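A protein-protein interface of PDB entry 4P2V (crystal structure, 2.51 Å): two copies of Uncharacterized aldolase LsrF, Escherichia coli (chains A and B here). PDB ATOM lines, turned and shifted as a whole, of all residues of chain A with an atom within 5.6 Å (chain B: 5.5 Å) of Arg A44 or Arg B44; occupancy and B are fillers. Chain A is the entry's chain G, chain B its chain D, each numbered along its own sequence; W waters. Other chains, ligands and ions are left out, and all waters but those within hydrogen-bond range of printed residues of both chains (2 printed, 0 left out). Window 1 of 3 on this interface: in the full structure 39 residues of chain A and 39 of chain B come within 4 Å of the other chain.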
ATOM      1  N   SER A  40      -2.108  -8.215  -3.220  1.00  0.00           N
ATOM      2  CA  SER A  40      -1.295  -7.430  -2.297  1.00  0.00           C
ATOM      3  C   SER A  40       0.176  -7.822  -2.334  1.00  0.00           C
ATOM      4  O   SER A  40       1.053  -6.957  -2.363  1.00  0.00           O
ATOM      5  CB  SER A  40      -1.818  -7.577  -0.871  1.00  0.00           C
ATOM      6  OG  SER A  40      -0.920  -6.997   0.057  1.00  0.00           O
ATOM      7  N   ARG A  41       0.436  -9.127  -2.325  1.00  0.00           N
ATOM      8  CA  ARG A  41       1.801  -9.642  -2.336  1.00  0.00           C
ATOM      9  C   ARG A  41       2.509  -9.284  -3.635  1.00  0.00           C
ATOM     10  O   ARG A  41       3.699  -8.984  -3.632  1.00  0.00           O
ATOM     11  CB  ARG A  41       1.815 -11.157  -2.131  1.00  0.00           C
ATOM     12  CG  ARG A  41       1.458 -11.591  -0.723  1.00  0.00           C
ATOM     13  CD  ARG A  41       1.651 -13.086  -0.530  1.00  0.00           C
ATOM     14  NE  ARG A  41       1.481 -13.472   0.869  1.00  0.00           N
ATOM     15  CZ  ARG A  41       0.338 -13.895   1.401  1.00  0.00           C
ATOM     16  NH1 ARG A  41      -0.749 -13.999   0.651  1.00  0.00           N
ATOM     17  NH2 ARG A  41       0.286 -14.217   2.687  1.00  0.00           N
ATOM     18  N   LEU A  42       1.779  -9.331  -4.745  1.00  0.00           N
ATOM     19  CA  LEU A  42       2.347  -8.955  -6.036  1.00  0.00           C
ATOM     20  C   LEU A  42       2.720  -7.474  -6.103  1.00  0.00           C
ATOM     21  O   LEU A  42       3.501  -7.068  -6.963  1.00  0.00           O
ATOM     22  CB  LEU A  42       1.409  -9.313  -7.188  1.00  0.00           C
ATOM     23  CG  LEU A  42       1.291 -10.804  -7.524  1.00  0.00           C
ATOM     24  CD1 LEU A  42       0.198 -11.043  -8.545  1.00  0.00           C
ATOM     25  CD2 LEU A  42       2.607 -11.379  -8.020  1.00  0.00           C
ATOM     26  N   SER A  43       2.123  -6.662  -5.235  1.00  0.00           N
ATOM     27  CA  SER A  43       2.437  -5.235  -5.200  1.00  0.00           C
ATOM     28  C   SER A  43       3.769  -4.964  -4.489  1.00  0.00           C
ATOM     29  O   SER A  43       4.425  -3.951  -4.748  1.00  0.00           O
ATOM     30  CB  SER A  43       1.307  -4.453  -4.521  1.00  0.00           C
ATOM     31  OG  SER A  43       0.113  -4.519  -5.283  1.00  0.00           O
ATOM     32  N   ARG A  44       4.185  -5.875  -3.614  1.00  0.00           N
ATOM     33  CA  ARG A  44       5.498  -5.753  -2.993  1.00  0.00           C
ATOM     34  C   ARG A  44       6.588  -6.107  -4.002  1.00  0.00           C
ATOM     35  O   ARG A  44       7.700  -5.580  -3.937  1.00  0.00           O
ATOM     36  CB  ARG A  44       5.615  -6.637  -1.745  1.00  0.00           C
ATOM     37  CG  ARG A  44       4.639  -6.281  -0.630  1.00  0.00           C
ATOM     38  CD  ARG A  44       5.061  -6.866   0.716  1.00  0.00           C
ATOM     39  NE  ARG A  44       6.304  -6.280   1.212  1.00  0.00           N
ATOM     40  CZ  ARG A  44       7.040  -6.802   2.190  1.00  0.00           C
ATOM     41  NH1 ARG A  44       6.662  -7.925   2.783  1.00  0.00           N
ATOM     42  NH2 ARG A  44       8.154  -6.195   2.578  1.00  0.00           N
ATOM     43  N   ILE A  45       6.272  -7.022  -4.914  1.00  0.00           N
ATOM     44  CA  ILE A  45       7.225  -7.452  -5.924  1.00  0.00           C
ATOM     45  C   ILE A  45       7.141  -6.524  -7.153  1.00  0.00           C
ATOM     46  O   ILE A  45       8.109  -5.830  -7.453  1.00  0.00           O
ATOM     47  CB  ILE A  45       7.035  -8.967  -6.215  1.00  0.00           C
ATOM     48  CG1 ILE A  45       5.661  -9.297  -6.800  1.00  0.00           C
ATOM     49  CG2 ILE A  45       7.269  -9.757  -4.908  1.00  0.00           C
ATOM     50  CD1 ILE A  45       5.696  -9.680  -8.256  1.00  0.00           C
ATOM     51  N   PHE A  46       5.996  -6.434  -7.820  1.00  0.00           N
ATOM     52  CA  PHE A  46       5.900  -5.486  -8.928  1.00  0.00           C
ATOM     53  C   PHE A  46       5.411  -4.157  -8.448  1.00  0.00           C
ATOM     54  O   PHE A  46       4.294  -4.035  -7.950  1.00  0.00           O
ATOM     55  CB  PHE A  46       5.001  -5.960 -10.041  1.00  0.00           C
ATOM     56  CG  PHE A  46       5.509  -7.146 -10.726  1.00  0.00           C
ATOM     57  CD1 PHE A  46       6.835  -7.228 -11.089  1.00  0.00           C
ATOM     58  CD2 PHE A  46       4.669  -8.183 -11.018  1.00  0.00           C
ATOM     59  CE1 PHE A  46       7.300  -8.332 -11.722  1.00  0.00           C
ATOM     60  CE2 PHE A  46       5.133  -9.278 -11.646  1.00  0.00           C
ATOM     61  CZ  PHE A  46       6.451  -9.354 -12.008  1.00  0.00           C
ATOM     62  N   ASN A  47       6.287  -3.173  -8.601  1.00  0.00           N
ATOM     63  CA  ASN A  47       6.047  -1.803  -8.191  1.00  0.00           C
ATOM     64  C   ASN A  47       4.792  -1.234  -8.878  1.00  0.00           C
ATOM     65  O   ASN A  47       4.680  -1.239 -10.107  1.00  0.00           O
ATOM     66  CB  ASN A  47       7.282  -0.953  -8.516  1.00  0.00           C
ATOM     67  CG  ASN A  47       7.155   0.479  -8.049  1.00  0.00           C
ATOM     68  OD1 ASN A  47       6.143   1.130  -8.265  1.00  0.00           O
ATOM     69  ND2 ASN A  47       8.214   0.988  -7.421  1.00  0.00           N
ATOM     70  N   ASP A  85      14.029  -4.436  -5.800  1.00  0.00           N
ATOM     71  CA  ASP A  85      12.650  -4.407  -5.309  1.00  0.00           C
ATOM     72  C   ASP A  85      12.356  -5.616  -4.419  1.00  0.00           C
ATOM     73  O   ASP A  85      11.732  -5.501  -3.357  1.00  0.00           O
ATOM     74  CB  ASP A  85      11.664  -4.323  -6.463  1.00  0.00           C
ATOM     75  CG  ASP A  85      11.736  -2.999  -7.149  1.00  0.00           C
ATOM     76  OD1 ASP A  85      12.252  -2.057  -6.513  1.00  0.00           O
ATOM     77  OD2 ASP A  85      11.286  -2.891  -8.299  1.00  0.00           O
ATOM     78  N   VAL A  86      12.844  -6.770  -4.853  1.00  0.00           N
ATOM     79  CA  VAL A  86      12.583  -8.030  -4.180  1.00  0.00           C
ATOM     80  C   VAL A  86      13.809  -8.920  -4.100  1.00  0.00           C
ATOM     81  O   VAL A  86      14.622  -8.959  -5.018  1.00  0.00           O
ATOM     82  CB  VAL A  86      11.473  -8.797  -4.890  1.00  0.00           C
ATOM     83  CG1 VAL A  86      10.178  -8.313  -4.418  1.00  0.00           C
ATOM     84  CG2 VAL A  86      11.565  -8.563  -6.380  1.00  0.00           C
ATOM     85  N   ASN A 103      13.619  -5.422   5.999  1.00  0.00           N
ATOM     86  CA  ASN A 103      12.291  -4.944   5.618  1.00  0.00           C
ATOM     87  C   ASN A 103      12.130  -4.950   4.115  1.00  0.00           C
ATOM     88  O   ASN A 103      11.906  -3.913   3.479  1.00  0.00           O
ATOM     89  CB  ASN A 103      12.021  -3.556   6.177  1.00  0.00           C
ATOM     90  CG  ASN A 103      10.571  -3.174   6.052  1.00  0.00           C
ATOM     91  OD1 ASN A 103       9.696  -4.039   5.982  1.00  0.00           O
ATOM     92  ND2 ASN A 103      10.302  -1.881   6.014  1.00  0.00           N
ATOM     93  N   ARG A 104      12.296  -6.137   3.553  1.00  0.00           N
ATOM     94  CA  ARG A 104      12.198  -6.288   2.126  1.00  0.00           C
ATOM     95  C   ARG A 104      11.330  -7.428   1.669  1.00  0.00           C
ATOM     96  O   ARG A 104      11.321  -8.483   2.302  1.00  0.00           O
ATOM     97  CB  ARG A 104      13.590  -6.512   1.603  1.00  0.00           C
ATOM     98  CG  ARG A 104      13.906  -5.585   0.564  1.00  0.00           C
ATOM     99  CD  ARG A 104      15.334  -5.333   0.669  1.00  0.00           C
ATOM    100  NE  ARG A 104      15.581  -4.201  -0.180  1.00  0.00           N
ATOM    101  CZ  ARG A 104      15.671  -4.287  -1.492  1.00  0.00           C
ATOM    102  NH1 ARG A 104      15.615  -5.465  -2.099  1.00  0.00           N
ATOM    103  NH2 ARG A 104      15.916  -3.193  -2.188  1.00  0.00           N
ATOM    104  N   PRO A 105      10.635  -7.239   0.541  1.00  0.00           N
ATOM    105  CA  PRO A 105       9.882  -8.358  -0.022  1.00  0.00           C
ATOM    106  C   PRO A 105      10.832  -9.519  -0.346  1.00  0.00           C
ATOM    107  O   PRO A 105      11.909  -9.304  -0.913  1.00  0.00           O
ATOM    108  CB  PRO A 105       9.270  -7.767  -1.288  1.00  0.00           C
ATOM    109  CG  PRO A 105       9.213  -6.294  -1.045  1.00  0.00           C
ATOM    110  CD  PRO A 105      10.397  -5.976  -0.179  1.00  0.00           C
ATOM    111  N   VAL A 106      10.429 -10.737  -0.002  1.00  0.00           N
ATOM    112  CA  VAL A 106      11.272 -11.905  -0.227  1.00  0.00           C
ATOM    113  C   VAL A 106      10.586 -12.947  -1.105  1.00  0.00           C
ATOM    114  O   VAL A 106       9.405 -13.249  -0.925  1.00  0.00           O
ATOM    115  CB  VAL A 106      11.686 -12.557   1.114  1.00  0.00           C
ATOM    116  CG1 VAL A 106      12.425 -13.865   0.877  1.00  0.00           C
ATOM    117  CG2 VAL A 106      12.547 -11.601   1.925  1.00  0.00           C
ATOM    118  N   ASN A 136       6.807 -15.235   5.988  1.00  0.00           N
ATOM    119  CA  ASN A 136       6.217 -14.048   5.375  1.00  0.00           C
ATOM    120  C   ASN A 136       6.732 -13.819   3.952  1.00  0.00           C
ATOM    121  O   ASN A 136       7.128 -12.711   3.591  1.00  0.00           O
ATOM    122  CB  ASN A 136       6.477 -12.809   6.244  1.00  0.00           C
ATOM    123  CG  ASN A 136       5.658 -11.606   5.809  1.00  0.00           C
ATOM    124  OD1 ASN A 136       4.525 -11.749   5.350  1.00  0.00           O
ATOM    125  ND2 ASN A 136       6.231 -10.416   5.949  1.00  0.00           N
ATOM    126  N   CYS A 138       6.620 -13.299  -0.100  1.00  0.00           N
ATOM    127  CA  CYS A 138       5.709 -12.610  -0.996  1.00  0.00           C
ATOM    128  C   CYS A 138       5.358 -13.558  -2.129  1.00  0.00           C
ATOM    129  O   CYS A 138       4.328 -13.407  -2.781  1.00  0.00           O
ATOM    130  CB  CYS A 138       6.330 -11.320  -1.532  1.00  0.00           C
ATOM    131  SG  CYS A 138       6.670 -10.077  -0.264  1.00  0.00           S
ATOM    132  N   SER B  40       9.928 -10.204  10.818  1.00  0.00           N
ATOM    133  CA  SER B  40       9.818  -9.576   9.501  1.00  0.00           C
ATOM    134  C   SER B  40       8.559  -8.714   9.370  1.00  0.00           C
ATOM    135  O   SER B  40       8.618  -7.589   8.874  1.00  0.00           O
ATOM    136  CB  SER B  40       9.830 -10.640   8.403  1.00  0.00           C
ATOM    137  OG  SER B  40       9.517 -10.073   7.144  1.00  0.00           O
ATOM    138  N   ARG B  41       7.424  -9.254   9.809  1.00  0.00           N
ATOM    139  CA  ARG B  41       6.145  -8.548   9.741  1.00  0.00           C
ATOM    140  C   ARG B  41       6.162  -7.327  10.653  1.00  0.00           C
ATOM    141  O   ARG B  41       5.589  -6.285  10.331  1.00  0.00           O
ATOM    142  CB  ARG B  41       4.986  -9.472  10.120  1.00  0.00           C
ATOM    143  CG  ARG B  41       4.680 -10.546   9.088  1.00  0.00           C
ATOM    144  CD  ARG B  41       3.423 -11.313   9.464  1.00  0.00           C
ATOM    145  NE  ARG B  41       3.014 -12.249   8.422  1.00  0.00           N
ATOM    146  CZ  ARG B  41       3.374 -13.527   8.387  1.00  0.00           C
ATOM    147  NH1 ARG B  41       4.158 -14.024   9.335  1.00  0.00           N
ATOM    148  NH2 ARG B  41       2.955 -14.312   7.404  1.00  0.00           N
ATOM    149  N   LEU B  42       6.810  -7.479  11.804  1.00  0.00           N
ATOM    150  CA  LEU B  42       6.952  -6.398  12.774  1.00  0.00           C
ATOM    151  C   LEU B  42       7.783  -5.242  12.225  1.00  0.00           C
ATOM    152  O   LEU B  42       7.659  -4.108  12.686  1.00  0.00           O
ATOM    153  CB  LEU B  42       7.582  -6.927  14.063  1.00  0.00           C
ATOM    154  CG  LEU B  42       6.690  -7.824  14.924  1.00  0.00           C
ATOM    155  CD1 LEU B  42       7.490  -8.464  16.045  1.00  0.00           C
ATOM    156  CD2 LEU B  42       5.520  -7.025  15.485  1.00  0.00           C
ATOM    157  N   SER B  43       8.636  -5.534  11.248  1.00  0.00           N
ATOM    158  CA  SER B  43       9.475  -4.510  10.635  1.00  0.00           C
ATOM    159  C   SER B  43       8.668  -3.674   9.647  1.00  0.00           C
ATOM    160  O   SER B  43       9.024  -2.534   9.347  1.00  0.00           O
ATOM    161  CB  SER B  43      10.674  -5.146   9.925  1.00  0.00           C
ATOM    162  OG  SER B  43      11.541  -5.786  10.846  1.00  0.00           O
ATOM    163  N   ARG B  44       7.574  -4.246   9.152  1.00  0.00           N
ATOM    164  CA  ARG B  44       6.665  -3.531   8.264  1.00  0.00           C
ATOM    165  C   ARG B  44       5.853  -2.495   9.034  1.00  0.00           C
ATOM    166  O   ARG B  44       5.520  -1.434   8.506  1.00  0.00           O
ATOM    167  CB  ARG B  44       5.734  -4.519   7.556  1.00  0.00           C
ATOM    168  CG  ARG B  44       6.460  -5.528   6.673  1.00  0.00           C
ATOM    169  CD  ARG B  44       5.515  -6.230   5.707  1.00  0.00           C
ATOM    170  NE  ARG B  44       4.935  -5.320   4.723  1.00  0.00           N
ATOM    171  CZ  ARG B  44       3.868  -5.603   3.984  1.00  0.00           C
ATOM    172  NH1 ARG B  44       3.256  -6.773   4.119  1.00  0.00           N
ATOM    173  NH2 ARG B  44       3.408  -4.715   3.112  1.00  0.00           N
ATOM    174  N   ILE B  45       5.544  -2.806  10.288  1.00  0.00           N
ATOM    175  CA  ILE B  45       4.779  -1.904  11.138  1.00  0.00           C
ATOM    176  C   ILE B  45       5.722  -0.896  11.764  1.00  0.00           C
ATOM    177  O   ILE B  45       5.608   0.310  11.551  1.00  0.00           O
ATOM    178  CB  ILE B  45       4.036  -2.654  12.254  1.00  0.00           C
ATOM    179  CG1 ILE B  45       3.052  -3.663  11.664  1.00  0.00           C
ATOM    180  CG2 ILE B  45       3.321  -1.671  13.168  1.00  0.00           C
ATOM    181  CD1 ILE B  45       2.552  -4.683  12.668  1.00  0.00           C
ATOM    182  N   PHE B  46       6.675  -1.422  12.520  1.00  0.00           N
ATOM    183  CA  PHE B  46       7.686  -0.618  13.184  1.00  0.00           C
ATOM    184  C   PHE B  46       8.890  -0.409  12.303  1.00  0.00           C
ATOM    185  O   PHE B  46       9.634  -1.337  11.990  1.00  0.00           O
ATOM    186  CB  PHE B  46       8.086  -1.275  14.498  1.00  0.00           C
ATOM    187  CG  PHE B  46       6.991  -1.285  15.496  1.00  0.00           C
ATOM    188  CD1 PHE B  46       6.306  -0.118  15.773  1.00  0.00           C
ATOM    189  CD2 PHE B  46       6.559  -2.464  16.067  1.00  0.00           C
ATOM    190  CE1 PHE B  46       5.276  -0.107  16.672  1.00  0.00           C
ATOM    191  CE2 PHE B  46       5.513  -2.458  16.956  1.00  0.00           C
ATOM    192  CZ  PHE B  46       4.876  -1.274  17.257  1.00  0.00           C
ATOM    193  N   ASN B  47       9.055   0.845  11.911  1.00  0.00           N
ATOM    194  CA  ASN B  47      10.137   1.273  11.051  1.00  0.00           C
ATOM    195  C   ASN B  47      11.493   0.913  11.668  1.00  0.00           C
ATOM    196  O   ASN B  47      11.777   1.285  12.805  1.00  0.00           O
ATOM    197  CB  ASN B  47      10.002   2.773  10.806  1.00  0.00           C
ATOM    198  CG  ASN B  47      11.088   3.318   9.925  1.00  0.00           C
ATOM    199  OD1 ASN B  47      12.235   3.444  10.342  1.00  0.00           O
ATOM    200  ND2 ASN B  47      10.735   3.638   8.687  1.00  0.00           N
ATOM    201  N   ASP B  85       2.144   4.662   7.659  1.00  0.00           N
ATOM    202  CA  ASP B  85       3.145   3.614   7.773  1.00  0.00           C
ATOM    203  C   ASP B  85       2.424   2.289   7.631  1.00  0.00           C
ATOM    204  O   ASP B  85       2.843   1.404   6.889  1.00  0.00           O
ATOM    205  CB  ASP B  85       3.875   3.684   9.115  1.00  0.00           C
ATOM    206  CG  ASP B  85       4.745   4.915   9.243  1.00  0.00           C
ATOM    207  OD1 ASP B  85       5.086   5.519   8.205  1.00  0.00           O
ATOM    208  OD2 ASP B  85       5.082   5.284  10.387  1.00  0.00           O
ATOM    209  N   VAL B  86       1.314   2.179   8.348  1.00  0.00           N
ATOM    210  CA  VAL B  86       0.516   0.969   8.356  1.00  0.00           C
ATOM    211  C   VAL B  86      -0.970   1.322   8.410  1.00  0.00           C
ATOM    212  O   VAL B  86      -1.374   2.237   9.129  1.00  0.00           O
ATOM    213  CB  VAL B  86       0.919   0.058   9.542  1.00  0.00           C
ATOM    214  CG1 VAL B  86       1.115   0.868  10.808  1.00  0.00           C
ATOM    215  CG2 VAL B  86      -0.073  -1.077   9.739  1.00  0.00           C
ATOM    216  N   ASN B 103      -0.088  -0.850  -1.467  1.00  0.00           N
ATOM    217  CA  ASN B 103       1.218  -1.319  -0.989  1.00  0.00           C
ATOM    218  C   ASN B 103       1.659  -0.774   0.379  1.00  0.00           C
ATOM    219  O   ASN B 103       2.722  -0.164   0.496  1.00  0.00           O
ATOM    220  CB  ASN B 103       2.285  -0.978  -2.050  1.00  0.00           C
ATOM    221  CG  ASN B 103       3.603  -1.719  -1.848  1.00  0.00           C
ATOM    222  OD1 ASN B 103       3.783  -2.454  -0.878  1.00  0.00           O
ATOM    223  ND2 ASN B 103       4.533  -1.523  -2.780  1.00  0.00           N
ATOM    224  N   ARG B 104       0.836  -0.985   1.406  1.00  0.00           N
ATOM    225  CA  ARG B 104       1.209  -0.650   2.785  1.00  0.00           C
ATOM    226  C   ARG B 104       0.906  -1.832   3.691  1.00  0.00           C
ATOM    227  O   ARG B 104      -0.001  -2.615   3.406  1.00  0.00           O
ATOM    228  CB  ARG B 104       0.454   0.564   3.339  1.00  0.00           C
ATOM    229  CG  ARG B 104      -0.134   1.502   2.333  1.00  0.00           C
ATOM    230  CD  ARG B 104       0.891   2.322   1.594  1.00  0.00           C
ATOM    231  NE  ARG B 104       1.808   3.022   2.479  1.00  0.00           N
ATOM    232  CZ  ARG B 104       2.811   3.778   2.048  1.00  0.00           C
ATOM    233  NH1 ARG B 104       3.019   3.924   0.746  1.00  0.00           N
ATOM    234  NH2 ARG B 104       3.600   4.387   2.919  1.00  0.00           N
ATOM    235  N   PRO B 105       1.670  -1.964   4.783  1.00  0.00           N
ATOM    236  CA  PRO B 105       1.395  -2.969   5.815  1.00  0.00           C
ATOM    237  C   PRO B 105      -0.017  -2.793   6.375  1.00  0.00           C
ATOM    238  O   PRO B 105      -0.448  -1.660   6.587  1.00  0.00           O
ATOM    239  CB  PRO B 105       2.446  -2.668   6.886  1.00  0.00           C
ATOM    240  CG  PRO B 105       3.550  -1.991   6.154  1.00  0.00           C
ATOM    241  CD  PRO B 105       2.915  -1.221   5.045  1.00  0.00           C
ATOM    242  N   VAL B 106      -0.730  -3.892   6.599  1.00  0.00           N
ATOM    243  CA  VAL B 106      -2.093  -3.824   7.121  1.00  0.00           C
ATOM    244  C   VAL B 106      -2.236  -4.587   8.442  1.00  0.00           C
ATOM    245  O   VAL B 106      -1.725  -5.698   8.583  1.00  0.00           O
ATOM    246  CB  VAL B 106      -3.112  -4.373   6.094  1.00  0.00           C
ATOM    247  CG1 VAL B 106      -4.508  -4.454   6.699  1.00  0.00           C
ATOM    248  CG2 VAL B 106      -3.124  -3.504   4.844  1.00  0.00           C
ATOM    249  N   ASN B 136      -2.471 -11.570   3.596  1.00  0.00           N
ATOM    250  CA  ASN B 136      -1.091 -11.152   3.847  1.00  0.00           C
ATOM    251  C   ASN B 136      -1.010 -10.050   4.901  1.00  0.00           C
ATOM    252  O   ASN B 136      -0.355  -9.027   4.700  1.00  0.00           O
ATOM    253  CB  ASN B 136      -0.415 -10.697   2.550  1.00  0.00           C
ATOM    254  CG  ASN B 136       1.085 -10.512   2.708  1.00  0.00           C
ATOM    255  OD1 ASN B 136       1.733 -11.226   3.474  1.00  0.00           O
ATOM    256  ND2 ASN B 136       1.640  -9.545   1.989  1.00  0.00           N
ATOM    257  N   CYS B 138      -0.022  -8.117   8.423  1.00  0.00           N
ATOM    258  CA  CYS B 138       1.198  -7.994   9.205  1.00  0.00           C
ATOM    259  C   CYS B 138       0.912  -8.285  10.670  1.00  0.00           C
ATOM    260  O   CYS B 138       1.817  -8.615  11.436  1.00  0.00           O
ATOM    261  CB  CYS B 138       1.803  -6.600   9.047  1.00  0.00           C
ATOM    262  SG  CYS B 138       2.337  -6.220   7.368  1.00  0.00           S
HETATM  263  O   HOH W   1       9.391  -6.882   6.143  1.00  0.00           O
HETATM  264  O   HOH W   2       3.553 -13.426   3.698  1.00  0.00           O
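Among the printed residues, pairs that only touch across the chains: Asn A136 with Ser B40 (3.5 Å), Arg A44 with Arg B44 (3.6 Å), Asn A103 with Arg B44 (3.6 Å), Asn A103 with Ser B43 (3.6 Å) and Arg A44 with Asn B103 (3.9 Å).
SG of Cys B138 is in hydrogen-bond range of NH1 of Arg B44 (3.4 Å). The side-chain sulfur of Cys A138 lies close to the guanidinium group of Arg A44, 3.7 Å away.
Of the printed residues of chain B, Arg A41 touches Asn B136 (3.4 Å). Printed residues of chain B within 4 Å of Ser A43: Asn B103. Arg A44 touches two residues of chain B. Of the printed residues of chain B, Asn A136 touches Ser B40 (3.5 Å), Arg B41 (3.5 Å) and Asn B136 (3.4 Å). Printed residues of chain A within 4 Å of Arg B41: Asn A136. Arg B44 touches just these residues of chain A: Arg A44 (3.6 Å) and Asn A103 (3.6 Å). The nearest residue of chain B that does not touch Arg A44 is Asn B136 (4.5 Å). The nearest residue of chain A that does not touch Arg B44 is Asn A136 (4.3 Å). The nearest printed residue of chain B that does not touch Arg A41 is Arg B41 (5.4 Å).
Water W2 bridges OD1 of Asn A136 (2.5 Å) and OD1 of Asn B136 (2.9 Å). Water W1 bridges OD1 of Asn A103 (2.9 Å) and O of Ser B40 (2.9 Å).
Printed residues of chain B that touch a printed residue of chain A: Ser B40, Arg B41, Ser B43, Arg B44, Asn B103 and Asn B136. Of the 16 printed residues of chain A, 5 touch a printed residue of chain B. Among the printed residues, 9 pairs touch across the chains. Among the printed residues, no Asp or Glu carboxylate lies within 4 Å of a Lys or Arg side-chain nitrogen of the other chain.
Arg A41 touches Asn B136, and with the chains exchanged Asn A136 touches Arg B41. Arg A44 touches Asn B103, and with the chains exchanged Asn A103 touches Arg B44. Asn A136 touches Ser B40, but with the chains exchanged Ser A40 does not touch Asn B136 (4.1 Å). Asn B136 touches its own counterpart, Asn A136. 16 positions are printed for both chains. Of the 9 pairs that touch across the chains among the printed residues, 8 have their exchanged pair printed and touching as well.
The side-chain amide oxygen of Asn A136 is in hydrogen-bond range of the guanidinium group of Arg B41 (3.5 Å). The side-chain amide nitrogen of Asn B103 sits at hydrogen-bond distance from the backbone carbonyl oxygen of Ser A43 (3.1 Å). The guanidinium group (NH2) of Arg A41 sits at hydrogen-bond distance from the side-chain amide oxygen (OD1) of Asn B136 (3.4 Å). The side-chain amide oxygen (OD1) of Asn B136 sits close to the side-chain amide oxygen (OD1) of Asn A136, 3.4 Å away.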
